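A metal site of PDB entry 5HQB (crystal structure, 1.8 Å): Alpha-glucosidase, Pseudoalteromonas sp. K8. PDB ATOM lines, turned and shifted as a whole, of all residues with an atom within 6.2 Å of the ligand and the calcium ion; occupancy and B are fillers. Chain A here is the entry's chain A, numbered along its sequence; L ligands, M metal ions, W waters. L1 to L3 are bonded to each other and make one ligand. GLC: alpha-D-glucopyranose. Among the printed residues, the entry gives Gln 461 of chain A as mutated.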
ATOM      1  N   TRP A 150     -32.103  -9.953   8.816  1.00  0.00           N
ATOM      2  CA  TRP A 150     -31.748 -11.307   9.207  1.00  0.00           C
ATOM      3  C   TRP A 150     -30.661 -11.332  10.268  1.00  0.00           C
ATOM      4  O   TRP A 150     -30.560 -12.309  11.028  1.00  0.00           O
ATOM      5  CB  TRP A 150     -31.303 -12.104   7.975  1.00  0.00           C
ATOM      6  CG  TRP A 150     -29.959 -11.689   7.443  1.00  0.00           C
ATOM      7  CD1 TRP A 150     -29.708 -10.698   6.534  1.00  0.00           C
ATOM      8  CD2 TRP A 150     -28.690 -12.238   7.805  1.00  0.00           C
ATOM      9  NE1 TRP A 150     -28.348 -10.599   6.311  1.00  0.00           N
ATOM     10  CE2 TRP A 150     -27.705 -11.536   7.076  1.00  0.00           C
ATOM     11  CE3 TRP A 150     -28.285 -13.258   8.666  1.00  0.00           C
ATOM     12  CZ2 TRP A 150     -26.342 -11.819   7.182  1.00  0.00           C
ATOM     13  CZ3 TRP A 150     -26.924 -13.554   8.776  1.00  0.00           C
ATOM     14  CH2 TRP A 150     -25.971 -12.834   8.038  1.00  0.00           C
ATOM     15  N   ASN A 151     -29.850 -10.278  10.370  1.00  0.00           N
ATOM     16  CA  ASN A 151     -28.766 -10.282  11.346  1.00  0.00           C
ATOM     17  C   ASN A 151     -28.995  -9.328  12.518  1.00  0.00           C
ATOM     18  O   ASN A 151     -28.032  -8.912  13.168  1.00  0.00           O
ATOM     19  CB  ASN A 151     -27.417  -9.974  10.668  1.00  0.00           C
ATOM     20  CG  ASN A 151     -26.289 -10.770  11.312  1.00  0.00           C
ATOM     21  OD1 ASN A 151     -26.524 -11.863  11.820  1.00  0.00           O
ATOM     22  ND2 ASN A 151     -25.092 -10.207  11.330  1.00  0.00           N
ATOM     23  N   ARG A 152     -30.254  -9.004  12.813  1.00  0.00           N
ATOM     24  CA  ARG A 152     -30.623  -8.367  14.090  1.00  0.00           C
ATOM     25  C   ARG A 152     -29.990  -6.988  14.210  1.00  0.00           C
ATOM     26  O   ARG A 152     -30.148  -6.162  13.313  1.00  0.00           O
ATOM     27  CB  ARG A 152     -30.233  -9.284  15.257  1.00  0.00           C
ATOM     28  CG  ARG A 152     -30.863 -10.707  15.143  1.00  0.00           C
ATOM     29  CD  ARG A 152     -30.362 -11.638  16.260  1.00  0.00           C
ATOM     30  NE  ARG A 152     -28.936 -11.424  16.410  1.00  0.00           N
ATOM     31  CZ  ARG A 152     -28.000 -11.994  15.669  1.00  0.00           C
ATOM     32  NH1 ARG A 152     -28.306 -12.927  14.770  1.00  0.00           N
ATOM     33  NH2 ARG A 152     -26.742 -11.646  15.856  1.00  0.00           N
ATOM     34  N   GLU A 154     -26.720  -6.536  14.287  1.00  0.00           N
ATOM     35  CA  GLU A 154     -25.314  -6.667  13.904  1.00  0.00           C
ATOM     36  C   GLU A 154     -25.139  -6.276  12.427  1.00  0.00           C
ATOM     37  O   GLU A 154     -24.970  -7.103  11.537  1.00  0.00           O
ATOM     38  CB  GLU A 154     -24.819  -8.091  14.180  1.00  0.00           C
ATOM     39  CG  GLU A 154     -24.645  -8.378  15.681  1.00  0.00           C
ATOM     40  CD  GLU A 154     -24.240  -9.826  15.943  1.00  0.00           C
ATOM     41  OE1 GLU A 154     -24.178 -10.611  14.978  1.00  0.00           O
ATOM     42  OE2 GLU A 154     -23.968 -10.156  17.114  1.00  0.00           O
ATOM     43  N   TRP A 270     -11.984 -18.279  23.529  1.00  0.00           N
ATOM     44  CA  TRP A 270     -13.023 -17.570  22.779  1.00  0.00           C
ATOM     45  C   TRP A 270     -12.528 -17.209  21.380  1.00  0.00           C
ATOM     46  O   TRP A 270     -13.004 -17.765  20.379  1.00  0.00           O
ATOM     47  CB  TRP A 270     -13.461 -16.300  23.543  1.00  0.00           C
ATOM     48  CG  TRP A 270     -14.495 -15.549  22.759  1.00  0.00           C
ATOM     49  CD1 TRP A 270     -15.790 -15.915  22.561  1.00  0.00           C
ATOM     50  CD2 TRP A 270     -14.297 -14.354  21.995  1.00  0.00           C
ATOM     51  NE1 TRP A 270     -16.424 -15.013  21.739  1.00  0.00           N
ATOM     52  CE2 TRP A 270     -15.522 -14.047  21.382  1.00  0.00           C
ATOM     53  CE3 TRP A 270     -13.203 -13.498  21.794  1.00  0.00           C
ATOM     54  CZ2 TRP A 270     -15.697 -12.919  20.555  1.00  0.00           C
ATOM     55  CZ3 TRP A 270     -13.369 -12.377  20.974  1.00  0.00           C
ATOM     56  CH2 TRP A 270     -14.611 -12.104  20.366  1.00  0.00           C
ATOM     57  N   HIS A 274     -13.029 -18.346  17.022  1.00  0.00           N
ATOM     58  CA  HIS A 274     -13.420 -17.451  15.931  1.00  0.00           C
ATOM     59  C   HIS A 274     -12.363 -17.384  14.835  1.00  0.00           C
ATOM     60  O   HIS A 274     -12.716 -17.157  13.672  1.00  0.00           O
ATOM     61  CB  HIS A 274     -13.736 -16.066  16.484  1.00  0.00           C
ATOM     62  CG  HIS A 274     -15.045 -16.014  17.189  1.00  0.00           C
ATOM     63  ND1 HIS A 274     -16.246 -15.871  16.523  1.00  0.00           N
ATOM     64  CD2 HIS A 274     -15.352 -16.182  18.501  1.00  0.00           C
ATOM     65  CE1 HIS A 274     -17.234 -15.909  17.410  1.00  0.00           C
ATOM     66  NE2 HIS A 274     -16.720 -16.088  18.610  1.00  0.00           N
ATOM     67  N   TRP A 280     -15.425 -25.152  19.169  1.00  0.00           N
ATOM     68  CA  TRP A 280     -16.349 -25.252  20.288  1.00  0.00           C
ATOM     69  C   TRP A 280     -16.677 -26.712  20.592  1.00  0.00           C
ATOM     70  O   TRP A 280     -16.818 -27.093  21.754  1.00  0.00           O
ATOM     71  CB  TRP A 280     -17.642 -24.509  20.008  1.00  0.00           C
ATOM     72  CG  TRP A 280     -17.599 -23.011  20.097  1.00  0.00           C
ATOM     73  CD1 TRP A 280     -17.808 -22.244  21.209  1.00  0.00           C
ATOM     74  CD2 TRP A 280     -17.382 -22.096  19.011  1.00  0.00           C
ATOM     75  NE1 TRP A 280     -17.720 -20.900  20.891  1.00  0.00           N
ATOM     76  CE2 TRP A 280     -17.458 -20.786  19.545  1.00  0.00           C
ATOM     77  CE3 TRP A 280     -17.124 -22.257  17.649  1.00  0.00           C
ATOM     78  CZ2 TRP A 280     -17.288 -19.637  18.759  1.00  0.00           C
ATOM     79  CZ3 TRP A 280     -16.949 -21.116  16.862  1.00  0.00           C
ATOM     80  CH2 TRP A 280     -17.032 -19.825  17.427  1.00  0.00           C
ATOM     81  N   GLU A 311     -16.054 -20.836  26.346  1.00  0.00           N
ATOM     82  CA  GLU A 311     -17.150 -21.290  25.510  1.00  0.00           C
ATOM     83  C   GLU A 311     -16.859 -22.691  24.986  1.00  0.00           C
ATOM     84  O   GLU A 311     -15.705 -23.053  24.724  1.00  0.00           O
ATOM     85  CB  GLU A 311     -17.379 -20.331  24.336  1.00  0.00           C
ATOM     86  CG  GLU A 311     -17.627 -18.908  24.784  1.00  0.00           C
ATOM     87  CD  GLU A 311     -18.148 -18.034  23.667  1.00  0.00           C
ATOM     88  OE1 GLU A 311     -18.152 -18.497  22.503  1.00  0.00           O
ATOM     89  OE2 GLU A 311     -18.559 -16.897  23.959  1.00  0.00           O
ATOM     90  N   TRP A 317     -22.368 -28.785  21.387  1.00  0.00           N
ATOM     91  CA  TRP A 317     -21.693 -27.975  20.372  1.00  0.00           C
ATOM     92  C   TRP A 317     -21.202 -28.785  19.174  1.00  0.00           C
ATOM     93  O   TRP A 317     -20.840 -28.178  18.156  1.00  0.00           O
ATOM     94  CB  TRP A 317     -20.495 -27.220  20.974  1.00  0.00           C
ATOM     95  CG  TRP A 317     -20.854 -26.129  21.948  1.00  0.00           C
ATOM     96  CD1 TRP A 317     -21.043 -26.261  23.303  1.00  0.00           C
ATOM     97  CD2 TRP A 317     -21.022 -24.732  21.664  1.00  0.00           C
ATOM     98  NE1 TRP A 317     -21.339 -25.050  23.866  1.00  0.00           N
ATOM     99  CE2 TRP A 317     -21.329 -24.088  22.880  1.00  0.00           C
ATOM    100  CE3 TRP A 317     -20.963 -23.962  20.498  1.00  0.00           C
ATOM    101  CZ2 TRP A 317     -21.569 -22.708  22.968  1.00  0.00           C
ATOM    102  CZ3 TRP A 317     -21.203 -22.592  20.577  1.00  0.00           C
ATOM    103  CH2 TRP A 317     -21.505 -21.982  21.808  1.00  0.00           C
ATOM    104  N   TRP A 321     -22.943 -25.801  15.458  1.00  0.00           N
ATOM    105  CA  TRP A 321     -23.666 -25.426  16.662  1.00  0.00           C
ATOM    106  C   TRP A 321     -24.792 -24.424  16.400  1.00  0.00           C
ATOM    107  O   TRP A 321     -25.702 -24.308  17.223  1.00  0.00           O
ATOM    108  CB  TRP A 321     -22.687 -24.866  17.698  1.00  0.00           C
ATOM    109  CG  TRP A 321     -21.932 -23.627  17.259  1.00  0.00           C
ATOM    110  CD1 TRP A 321     -20.661 -23.593  16.713  1.00  0.00           C
ATOM    111  CD2 TRP A 321     -22.369 -22.261  17.347  1.00  0.00           C
ATOM    112  NE1 TRP A 321     -20.304 -22.283  16.455  1.00  0.00           N
ATOM    113  CE2 TRP A 321     -21.335 -21.457  16.839  1.00  0.00           C
ATOM    114  CE3 TRP A 321     -23.542 -21.649  17.807  1.00  0.00           C
ATOM    115  CZ2 TRP A 321     -21.433 -20.062  16.772  1.00  0.00           C
ATOM    116  CZ3 TRP A 321     -23.643 -20.266  17.744  1.00  0.00           C
ATOM    117  CH2 TRP A 321     -22.592 -19.485  17.219  1.00  0.00           C
ATOM    118  N   PHE A 322     -24.741 -23.708  15.273  1.00  0.00           N
ATOM    119  CA  PHE A 322     -25.838 -22.803  14.907  1.00  0.00           C
ATOM    120  C   PHE A 322     -27.187 -23.517  14.889  1.00  0.00           C
ATOM    121  O   PHE A 322     -28.229 -22.902  15.167  1.00  0.00           O
ATOM    122  CB  PHE A 322     -25.543 -22.177  13.538  1.00  0.00           C
ATOM    123  CG  PHE A 322     -26.582 -21.171  13.071  1.00  0.00           C
ATOM    124  CD1 PHE A 322     -27.669 -21.573  12.315  1.00  0.00           C
ATOM    125  CD2 PHE A 322     -26.424 -19.820  13.368  1.00  0.00           C
ATOM    126  CE1 PHE A 322     -28.612 -20.645  11.878  1.00  0.00           C
ATOM    127  CE2 PHE A 322     -27.367 -18.891  12.931  1.00  0.00           C
ATOM    128  CZ  PHE A 322     -28.464 -19.301  12.193  1.00  0.00           C
ATOM    129  N   HIS A 356     -21.067 -19.594  30.466  1.00  0.00           N
ATOM    130  CA  HIS A 356     -21.539 -19.349  29.111  1.00  0.00           C
ATOM    131  C   HIS A 356     -22.744 -20.227  28.819  1.00  0.00           C
ATOM    132  O   HIS A 356     -22.660 -21.456  28.956  1.00  0.00           O
ATOM    133  CB  HIS A 356     -20.427 -19.640  28.087  1.00  0.00           C
ATOM    134  CG  HIS A 356     -20.805 -19.247  26.684  1.00  0.00           C
ATOM    135  ND1 HIS A 356     -20.672 -20.094  25.607  1.00  0.00           N
ATOM    136  CD2 HIS A 356     -21.311 -18.088  26.196  1.00  0.00           C
ATOM    137  CE1 HIS A 356     -21.082 -19.482  24.511  1.00  0.00           C
ATOM    138  NE2 HIS A 356     -21.463 -18.265  24.841  1.00  0.00           N
ATOM    139  N   GLU A 358     -25.014 -20.472  25.613  1.00  0.00           N
ATOM    140  CA  GLU A 358     -25.495 -20.220  24.251  1.00  0.00           C
ATOM    141  C   GLU A 358     -26.748 -21.050  24.012  1.00  0.00           C
ATOM    142  O   GLU A 358     -26.748 -22.258  24.264  1.00  0.00           O
ATOM    143  CB  GLU A 358     -24.421 -20.564  23.223  1.00  0.00           C
ATOM    144  CG  GLU A 358     -24.903 -20.474  21.774  1.00  0.00           C
ATOM    145  CD  GLU A 358     -25.346 -19.066  21.401  1.00  0.00           C
ATOM    146  OE1 GLU A 358     -24.503 -18.146  21.428  1.00  0.00           O
ATOM    147  OE2 GLU A 358     -26.540 -18.871  21.085  1.00  0.00           O
ATOM    148  N   LYS A 386     -22.087 -15.173  30.477  1.00  0.00           N
ATOM    149  CA  LYS A 386     -22.387 -14.668  29.149  1.00  0.00           C
ATOM    150  C   LYS A 386     -23.465 -15.539  28.534  1.00  0.00           C
ATOM    151  O   LYS A 386     -23.324 -16.760  28.485  1.00  0.00           O
ATOM    152  CB  LYS A 386     -21.123 -14.701  28.279  1.00  0.00           C
ATOM    153  CG  LYS A 386     -21.320 -14.251  26.832  1.00  0.00           C
ATOM    154  CD  LYS A 386     -19.983 -14.386  26.092  1.00  0.00           C
ATOM    155  CE  LYS A 386     -20.121 -13.993  24.621  1.00  0.00           C
ATOM    156  NZ  LYS A 386     -18.871 -14.253  23.861  1.00  0.00           N
ATOM    157  N   GLY A 388     -26.307 -16.225  25.195  1.00  0.00           N
ATOM    158  CA  GLY A 388     -26.339 -16.086  23.745  1.00  0.00           C
ATOM    159  C   GLY A 388     -27.659 -16.557  23.183  1.00  0.00           C
ATOM    160  O   GLY A 388     -28.282 -17.484  23.698  1.00  0.00           O
ATOM    161  N   VAL A 390     -28.195 -17.013  19.444  1.00  0.00           N
ATOM    162  CA  VAL A 390     -27.804 -16.958  18.034  1.00  0.00           C
ATOM    163  C   VAL A 390     -28.888 -17.597  17.168  1.00  0.00           C
ATOM    164  O   VAL A 390     -29.113 -18.809  17.212  1.00  0.00           O
ATOM    165  CB  VAL A 390     -26.442 -17.635  17.804  1.00  0.00           C
ATOM    166  CG1 VAL A 390     -26.126 -17.691  16.306  1.00  0.00           C
ATOM    167  CG2 VAL A 390     -25.360 -16.881  18.556  1.00  0.00           C
ATOM    168  N   ALA A 391     -29.540 -16.762  16.357  1.00  0.00           N
ATOM    169  CA  ALA A 391     -30.538 -17.167  15.373  1.00  0.00           C
ATOM    170  C   ALA A 391     -30.800 -15.954  14.497  1.00  0.00           C
ATOM    171  O   ALA A 391     -30.593 -14.811  14.933  1.00  0.00           O
ATOM    172  CB  ALA A 391     -31.845 -17.636  16.046  1.00  0.00           C
ATOM    173  N   ASP A 392     -31.237 -16.187  13.272  1.00  0.00           N
ATOM    174  CA  ASP A 392     -31.549 -15.070  12.397  1.00  0.00           C
ATOM    175  C   ASP A 392     -32.723 -14.263  12.950  1.00  0.00           C
ATOM    176  O   ASP A 392     -33.490 -14.737  13.802  1.00  0.00           O
ATOM    177  CB  ASP A 392     -31.880 -15.553  10.982  1.00  0.00           C
ATOM    178  CG  ASP A 392     -30.662 -16.000  10.206  1.00  0.00           C
ATOM    179  OD1 ASP A 392     -29.535 -15.998  10.758  1.00  0.00           O
ATOM    180  OD2 ASP A 392     -30.834 -16.357   9.014  1.00  0.00           O
ATOM    181  N   HIS A 436     -25.332 -11.604  24.804  1.00  0.00           N
ATOM    182  CA  HIS A 436     -25.126 -11.476  23.371  1.00  0.00           C
ATOM    183  C   HIS A 436     -26.421 -11.832  22.633  1.00  0.00           C
ATOM    184  O   HIS A 436     -27.258 -12.576  23.144  1.00  0.00           O
ATOM    185  CB  HIS A 436     -23.942 -12.333  22.904  1.00  0.00           C
ATOM    186  CG  HIS A 436     -22.615 -11.705  23.244  1.00  0.00           C
ATOM    187  ND1 HIS A 436     -21.551 -11.698  22.379  1.00  0.00           N
ATOM    188  CD2 HIS A 436     -22.221 -11.012  24.349  1.00  0.00           C
ATOM    189  CE1 HIS A 436     -20.545 -11.041  22.934  1.00  0.00           C
ATOM    190  NE2 HIS A 436     -20.922 -10.615  24.128  1.00  0.00           N
ATOM    191  N   GLU A 437     -26.567 -11.292  21.419  1.00  0.00           N
ATOM    192  CA  GLU A 437     -27.837 -11.236  20.694  1.00  0.00           C
ATOM    193  C   GLU A 437     -28.972 -10.822  21.638  1.00  0.00           C
ATOM    194  O   GLU A 437     -29.914 -11.577  21.872  1.00  0.00           O
ATOM    195  CB  GLU A 437     -28.151 -12.567  20.015  1.00  0.00           C
ATOM    196  CG  GLU A 437     -27.063 -13.013  19.034  1.00  0.00           C
ATOM    197  CD  GLU A 437     -25.821 -13.550  19.739  1.00  0.00           C
ATOM    198  OE1 GLU A 437     -25.972 -14.303  20.731  1.00  0.00           O
ATOM    199  OE2 GLU A 437     -24.693 -13.220  19.313  1.00  0.00           O
ATOM    200  N   GLU A 455     -24.076  -7.251  23.927  1.00  0.00           N
ATOM    201  CA  GLU A 455     -23.501  -6.984  22.616  1.00  0.00           C
ATOM    202  C   GLU A 455     -24.475  -6.141  21.803  1.00  0.00           C
ATOM    203  O   GLU A 455     -24.527  -4.921  21.977  1.00  0.00           O
ATOM    204  CB  GLU A 455     -23.145  -8.292  21.896  1.00  0.00           C
ATOM    205  CG  GLU A 455     -22.235  -8.086  20.695  1.00  0.00           C
ATOM    206  CD  GLU A 455     -21.847  -9.396  20.038  1.00  0.00           C
ATOM    207  OE1 GLU A 455     -22.761 -10.193  19.725  1.00  0.00           O
ATOM    208  OE2 GLU A 455     -20.642  -9.625  19.850  1.00  0.00           O
ATOM    209  N   ALA A 457     -24.728  -5.336  18.539  1.00  0.00           N
ATOM    210  CA  ALA A 457     -24.060  -4.520  17.538  1.00  0.00           C
ATOM    211  C   ALA A 457     -22.887  -5.358  17.051  1.00  0.00           C
ATOM    212  O   ALA A 457     -22.516  -6.355  17.669  1.00  0.00           O
ATOM    213  CB  ALA A 457     -23.558  -3.176  18.105  1.00  0.00           C
ATOM    214  N   GLN A 461     -15.784  -9.735  16.988  1.00  0.00           N
ATOM    215  CA  GLN A 461     -15.906 -11.033  16.321  1.00  0.00           C
ATOM    216  C   GLN A 461     -16.064 -10.886  14.814  1.00  0.00           C
ATOM    217  O   GLN A 461     -15.596 -11.752  14.062  1.00  0.00           O
ATOM    218  CB  GLN A 461     -17.099 -11.827  16.884  1.00  0.00           C
ATOM    219  CG  GLN A 461     -18.458 -11.161  16.657  1.00  0.00           C
ATOM    220  CD  GLN A 461     -19.643 -12.039  17.020  1.00  0.00           C
ATOM    221  OE1 GLN A 461     -20.763 -11.543  17.178  1.00  0.00           O
ATOM    222  NE2 GLN A 461     -19.415 -13.348  17.136  1.00  0.00           N
ATOM    223  N   PHE A 462     -16.702  -9.801  14.346  1.00  0.00           N
ATOM    224  CA  PHE A 462     -16.824  -9.630  12.895  1.00  0.00           C
ATOM    225  C   PHE A 462     -15.493  -9.354  12.221  1.00  0.00           C
ATOM    226  O   PHE A 462     -15.416  -9.434  10.985  1.00  0.00           O
ATOM    227  CB  PHE A 462     -17.833  -8.524  12.580  1.00  0.00           C
ATOM    228  CG  PHE A 462     -19.247  -8.984  12.716  1.00  0.00           C
ATOM    229  CD1 PHE A 462     -19.852  -9.076  13.965  1.00  0.00           C
ATOM    230  CD2 PHE A 462     -19.941  -9.414  11.596  1.00  0.00           C
ATOM    231  CE1 PHE A 462     -21.155  -9.554  14.086  1.00  0.00           C
ATOM    232  CE2 PHE A 462     -21.247  -9.881  11.705  1.00  0.00           C
ATOM    233  CZ  PHE A 462     -21.839  -9.967  12.956  1.00  0.00           C
ATOM    234  N   TRP A 465     -14.119 -12.913  10.763  1.00  0.00           N
ATOM    235  CA  TRP A 465     -14.718 -13.621   9.628  1.00  0.00           C
ATOM    236  C   TRP A 465     -15.784 -12.803   8.896  1.00  0.00           C
ATOM    237  O   TRP A 465     -16.506 -13.387   8.068  1.00  0.00           O
ATOM    238  CB  TRP A 465     -15.347 -14.959  10.119  1.00  0.00           C
ATOM    239  CG  TRP A 465     -16.018 -14.849  11.473  1.00  0.00           C
ATOM    240  CD1 TRP A 465     -15.562 -15.344  12.661  1.00  0.00           C
ATOM    241  CD2 TRP A 465     -17.243 -14.165  11.785  1.00  0.00           C
ATOM    242  NE1 TRP A 465     -16.416 -15.028  13.684  1.00  0.00           N
ATOM    243  CE2 TRP A 465     -17.462 -14.306  13.170  1.00  0.00           C
ATOM    244  CE3 TRP A 465     -18.180 -13.456  11.023  1.00  0.00           C
ATOM    245  CZ2 TRP A 465     -18.571 -13.762  13.817  1.00  0.00           C
ATOM    246  CZ3 TRP A 465     -19.294 -12.914  11.662  1.00  0.00           C
ATOM    247  CH2 TRP A 465     -19.474 -13.068  13.050  1.00  0.00           C
ATOM    248  N   GLY A 466     -15.902 -11.490   9.138  1.00  0.00           N
ATOM    249  CA  GLY A 466     -17.085 -10.759   8.690  1.00  0.00           C
ATOM    250  C   GLY A 466     -17.285 -10.771   7.179  1.00  0.00           C
ATOM    251  O   GLY A 466     -18.426 -10.837   6.706  1.00  0.00           O
ATOM    252  N   THR A 491     -15.375  -6.664  23.141  1.00  0.00           N
ATOM    253  CA  THR A 491     -14.165  -7.508  23.232  1.00  0.00           C
ATOM    254  C   THR A 491     -13.016  -6.830  22.482  1.00  0.00           C
ATOM    255  O   THR A 491     -12.563  -7.314  21.442  1.00  0.00           O
ATOM    256  CB  THR A 491     -14.401  -8.959  22.753  1.00  0.00           C
ATOM    257  OG1 THR A 491     -14.450  -9.037  21.320  1.00  0.00           O
ATOM    258  CG2 THR A 491     -15.703  -9.517  23.335  1.00  0.00           C
HETATM  259  C1  GLC L   1     -19.685 -17.625  10.064  1.00  0.00           C
HETATM  260  C2  GLC L   1     -20.952 -17.030   9.433  1.00  0.00           C
HETATM  261  C3  GLC L   1     -21.735 -16.144  10.401  1.00  0.00           C
HETATM  262  C4  GLC L   1     -21.630 -16.621  11.848  1.00  0.00           C
HETATM  263  C5  GLC L   1     -20.166 -16.818  12.254  1.00  0.00           C
HETATM  264  C6  GLC L   1     -19.991 -18.122  13.021  1.00  0.00           C
HETATM  265  O2  GLC L   1     -20.599 -16.276   8.300  1.00  0.00           O
HETATM  266  O3  GLC L   1     -23.109 -16.132  10.037  1.00  0.00           O
HETATM  267  O4  GLC L   1     -22.263 -15.648  12.676  1.00  0.00           O
HETATM  268  O5  GLC L   1     -19.277 -16.819  11.151  1.00  0.00           O
HETATM  269  O6  GLC L   1     -19.741 -17.810  14.364  1.00  0.00           O
HETATM  270  C1  GLC L   2     -23.353 -16.249  13.424  1.00  0.00           C
HETATM  271  C2  GLC L   2     -24.595 -15.337  13.387  1.00  0.00           C
HETATM  272  C3  GLC L   2     -24.270 -13.995  14.033  1.00  0.00           C
HETATM  273  C4  GLC L   2     -23.773 -14.226  15.476  1.00  0.00           C
HETATM  274  C5  GLC L   2     -22.630 -15.258  15.500  1.00  0.00           C
HETATM  275  C6  GLC L   2     -22.307 -15.773  16.910  1.00  0.00           C
HETATM  276  O2  GLC L   2     -25.034 -15.214  12.048  1.00  0.00           O
HETATM  277  O3  GLC L   2     -25.405 -13.133  14.025  1.00  0.00           O
HETATM  278  O4  GLC L   2     -23.353 -13.009  16.067  1.00  0.00           O
HETATM  279  O5  GLC L   2     -22.995 -16.418  14.784  1.00  0.00           O
HETATM  280  O6  GLC L   2     -21.687 -14.873  17.797  1.00  0.00           O
HETATM  281  C1  GLC L   3     -22.180 -15.191  19.141  1.00  0.00           C
HETATM  282  C2  GLC L   3     -21.428 -14.381  20.214  1.00  0.00           C
HETATM  283  C3  GLC L   3     -19.948 -14.761  20.223  1.00  0.00           C
HETATM  284  C4  GLC L   3     -19.884 -16.233  20.665  1.00  0.00           C
HETATM  285  C5  GLC L   3     -20.742 -17.121  19.761  1.00  0.00           C
HETATM  286  C6  GLC L   3     -20.967 -18.500  20.401  1.00  0.00           C
HETATM  287  O2  GLC L   3     -21.629 -12.993  20.032  1.00  0.00           O
HETATM  288  O3  GLC L   3     -19.232 -13.899  21.096  1.00  0.00           O
HETATM  289  O4  GLC L   3     -18.549 -16.699  20.645  1.00  0.00           O
HETATM  290  O5  GLC L   3     -22.033 -16.580  19.460  1.00  0.00           O
HETATM  291  O6  GLC L   3     -21.757 -18.397  21.579  1.00  0.00           O
HETATM  292 CA    CA M   1     -22.979 -12.014  18.157  1.00  0.00          CA
HETATM  293  O   HOH W   1     -22.728 -19.666  13.651  1.00  0.00           O
HETATM  294  O   HOH W   2     -23.424 -15.558   6.711  1.00  0.00           O
HETATM  295  O   HOH W   3     -23.320 -12.759  10.773  1.00  0.00           O
HETATM  296  O   HOH W   4     -19.255 -14.419   7.001  1.00  0.00           O
HETATM  297  O   HOH W   5     -27.650 -14.461  12.101  1.00  0.00           O
HETATM  298  O   HOH W   6     -23.968 -15.660  21.594  1.00  0.00           O
HETATM  299  O   HOH W   7     -18.805 -11.483  19.967  1.00  0.00           O
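Water W4 lies within hydrogen-bond range of an oxygen (O2) of GLC L1 (2.6 Å) and the backbone carbonyl oxygen (O) of Trp 465 (3.1 Å).
Water W7 lies within hydrogen-bond range of OE2 of Glu 455 (2.6 Å), O3 of GLC L3 (2.7 Å) and NE2 of Gln 461 (3.4 Å).
Water W5 lies within hydrogen-bond range of an oxygen (O2) of GLC L2, the side-chain carboxylate (OD1) of Asp 392, the side-chain amide oxygen (OD1) of Asn 151 and the guanidinium group (NH1) of Arg 152.
Water W3 bridges the side-chain amide nitrogen of Asn 151 (3.2 Å) and an oxygen (O2) of GLC L2 (3.3 Å).
Four residues have an atom within 4 Å of the calcium ion: Glu 154, Glu 437, Glu 455 and Gln 461.
The nearest printed residue that does not touch the calcium ion is Arg 152 (4.4 Å).
The guanidinium group of Arg 152 lies within salt-bridge range of the side-chain carboxylate of Glu 154.
The backbone carbonyl oxygen (O) of Glu 154 sits at hydrogen-bond distance from the side-chain amide nitrogen (ND2) of Asn 151.
The indole nitrogen of Trp 465 lies close to the backbone carbonyl oxygen of Gln 461, at 3.4 Å.
The side-chain carboxylate of Glu 311 is in salt-bridge range of the side-chain amino group of Lys 386 (2.7 Å).
OE1 of Glu 311 is in hydrogen-bond range of NE1 of Trp 280.
The backbone carbonyl oxygen (O) of Ala 391 sits at hydrogen-bond distance from the guanidinium group (NH1) of Arg 152 (3.0 Å).
N of Val 390 is in hydrogen-bond range of OE2 of Glu 358, 3.0 Å away.
A ring nitrogen (ND1) of His 274 sits at hydrogen-bond distance from the indole nitrogen of Trp 465 (3.0 Å).
OE1 of Glu 311 lies within hydrogen-bond range of O4 of GLC L3 (2.6 Å).
O3 of GLC L3 is in hydrogen-bond range of ND1 of His 436.
An oxygen (O3) of GLC L2 is in hydrogen-bond range of the guanidinium group of Arg 152 (2.7 Å).
OE1 of Glu 358 lies within hydrogen-bond range of O6 of GLC L3, 2.8 Å away.
OD1 of Asn 151 lies within hydrogen-bond range of O3 of GLC L2 (2.8 Å).
A ring nitrogen (NE2) of His 274 sits at hydrogen-bond distance from an oxygen (O4) of GLC L3, 2.8 Å away.
O3 of GLC L3 lies within hydrogen-bond range of NZ of Lys 386, 2.8 Å away.
An oxygen (O4) of GLC L3 lies within hydrogen-bond range of the indole nitrogen (NE1) of Trp 270 (2.9 Å).
A ring nitrogen (NE2) of His 356 lies close to an oxygen (O6) of GLC L3, 3.3 Å away.
The calcium ion is bound by an oxygen (O4) of GLC L2 (2.3 Å), the side-chain carboxylate of Glu 154 (2.3 Å), the side-chain carboxylate of Glu 437 (2.4 Å), the side-chain carboxylate of Glu 455 (2.4 Å), the side-chain amide oxygen of Gln 461 (2.5 Å) and an oxygen (O2) of GLC L3 (2.5 Å).
Trp 280 touches the ligand.
CH2 of Trp 317 touches O6 of GLC L3, at 3.6 Å.
Trp 321 touches the ligand.
CG2 of Val 390 touches O5 of GLC L3 (3.5 Å).
CD2 of Trp 465 touches O5 of GLC L1 (3.4 Å).
Of the 27 residues printed, 18 come within 4 Å of the ligand.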
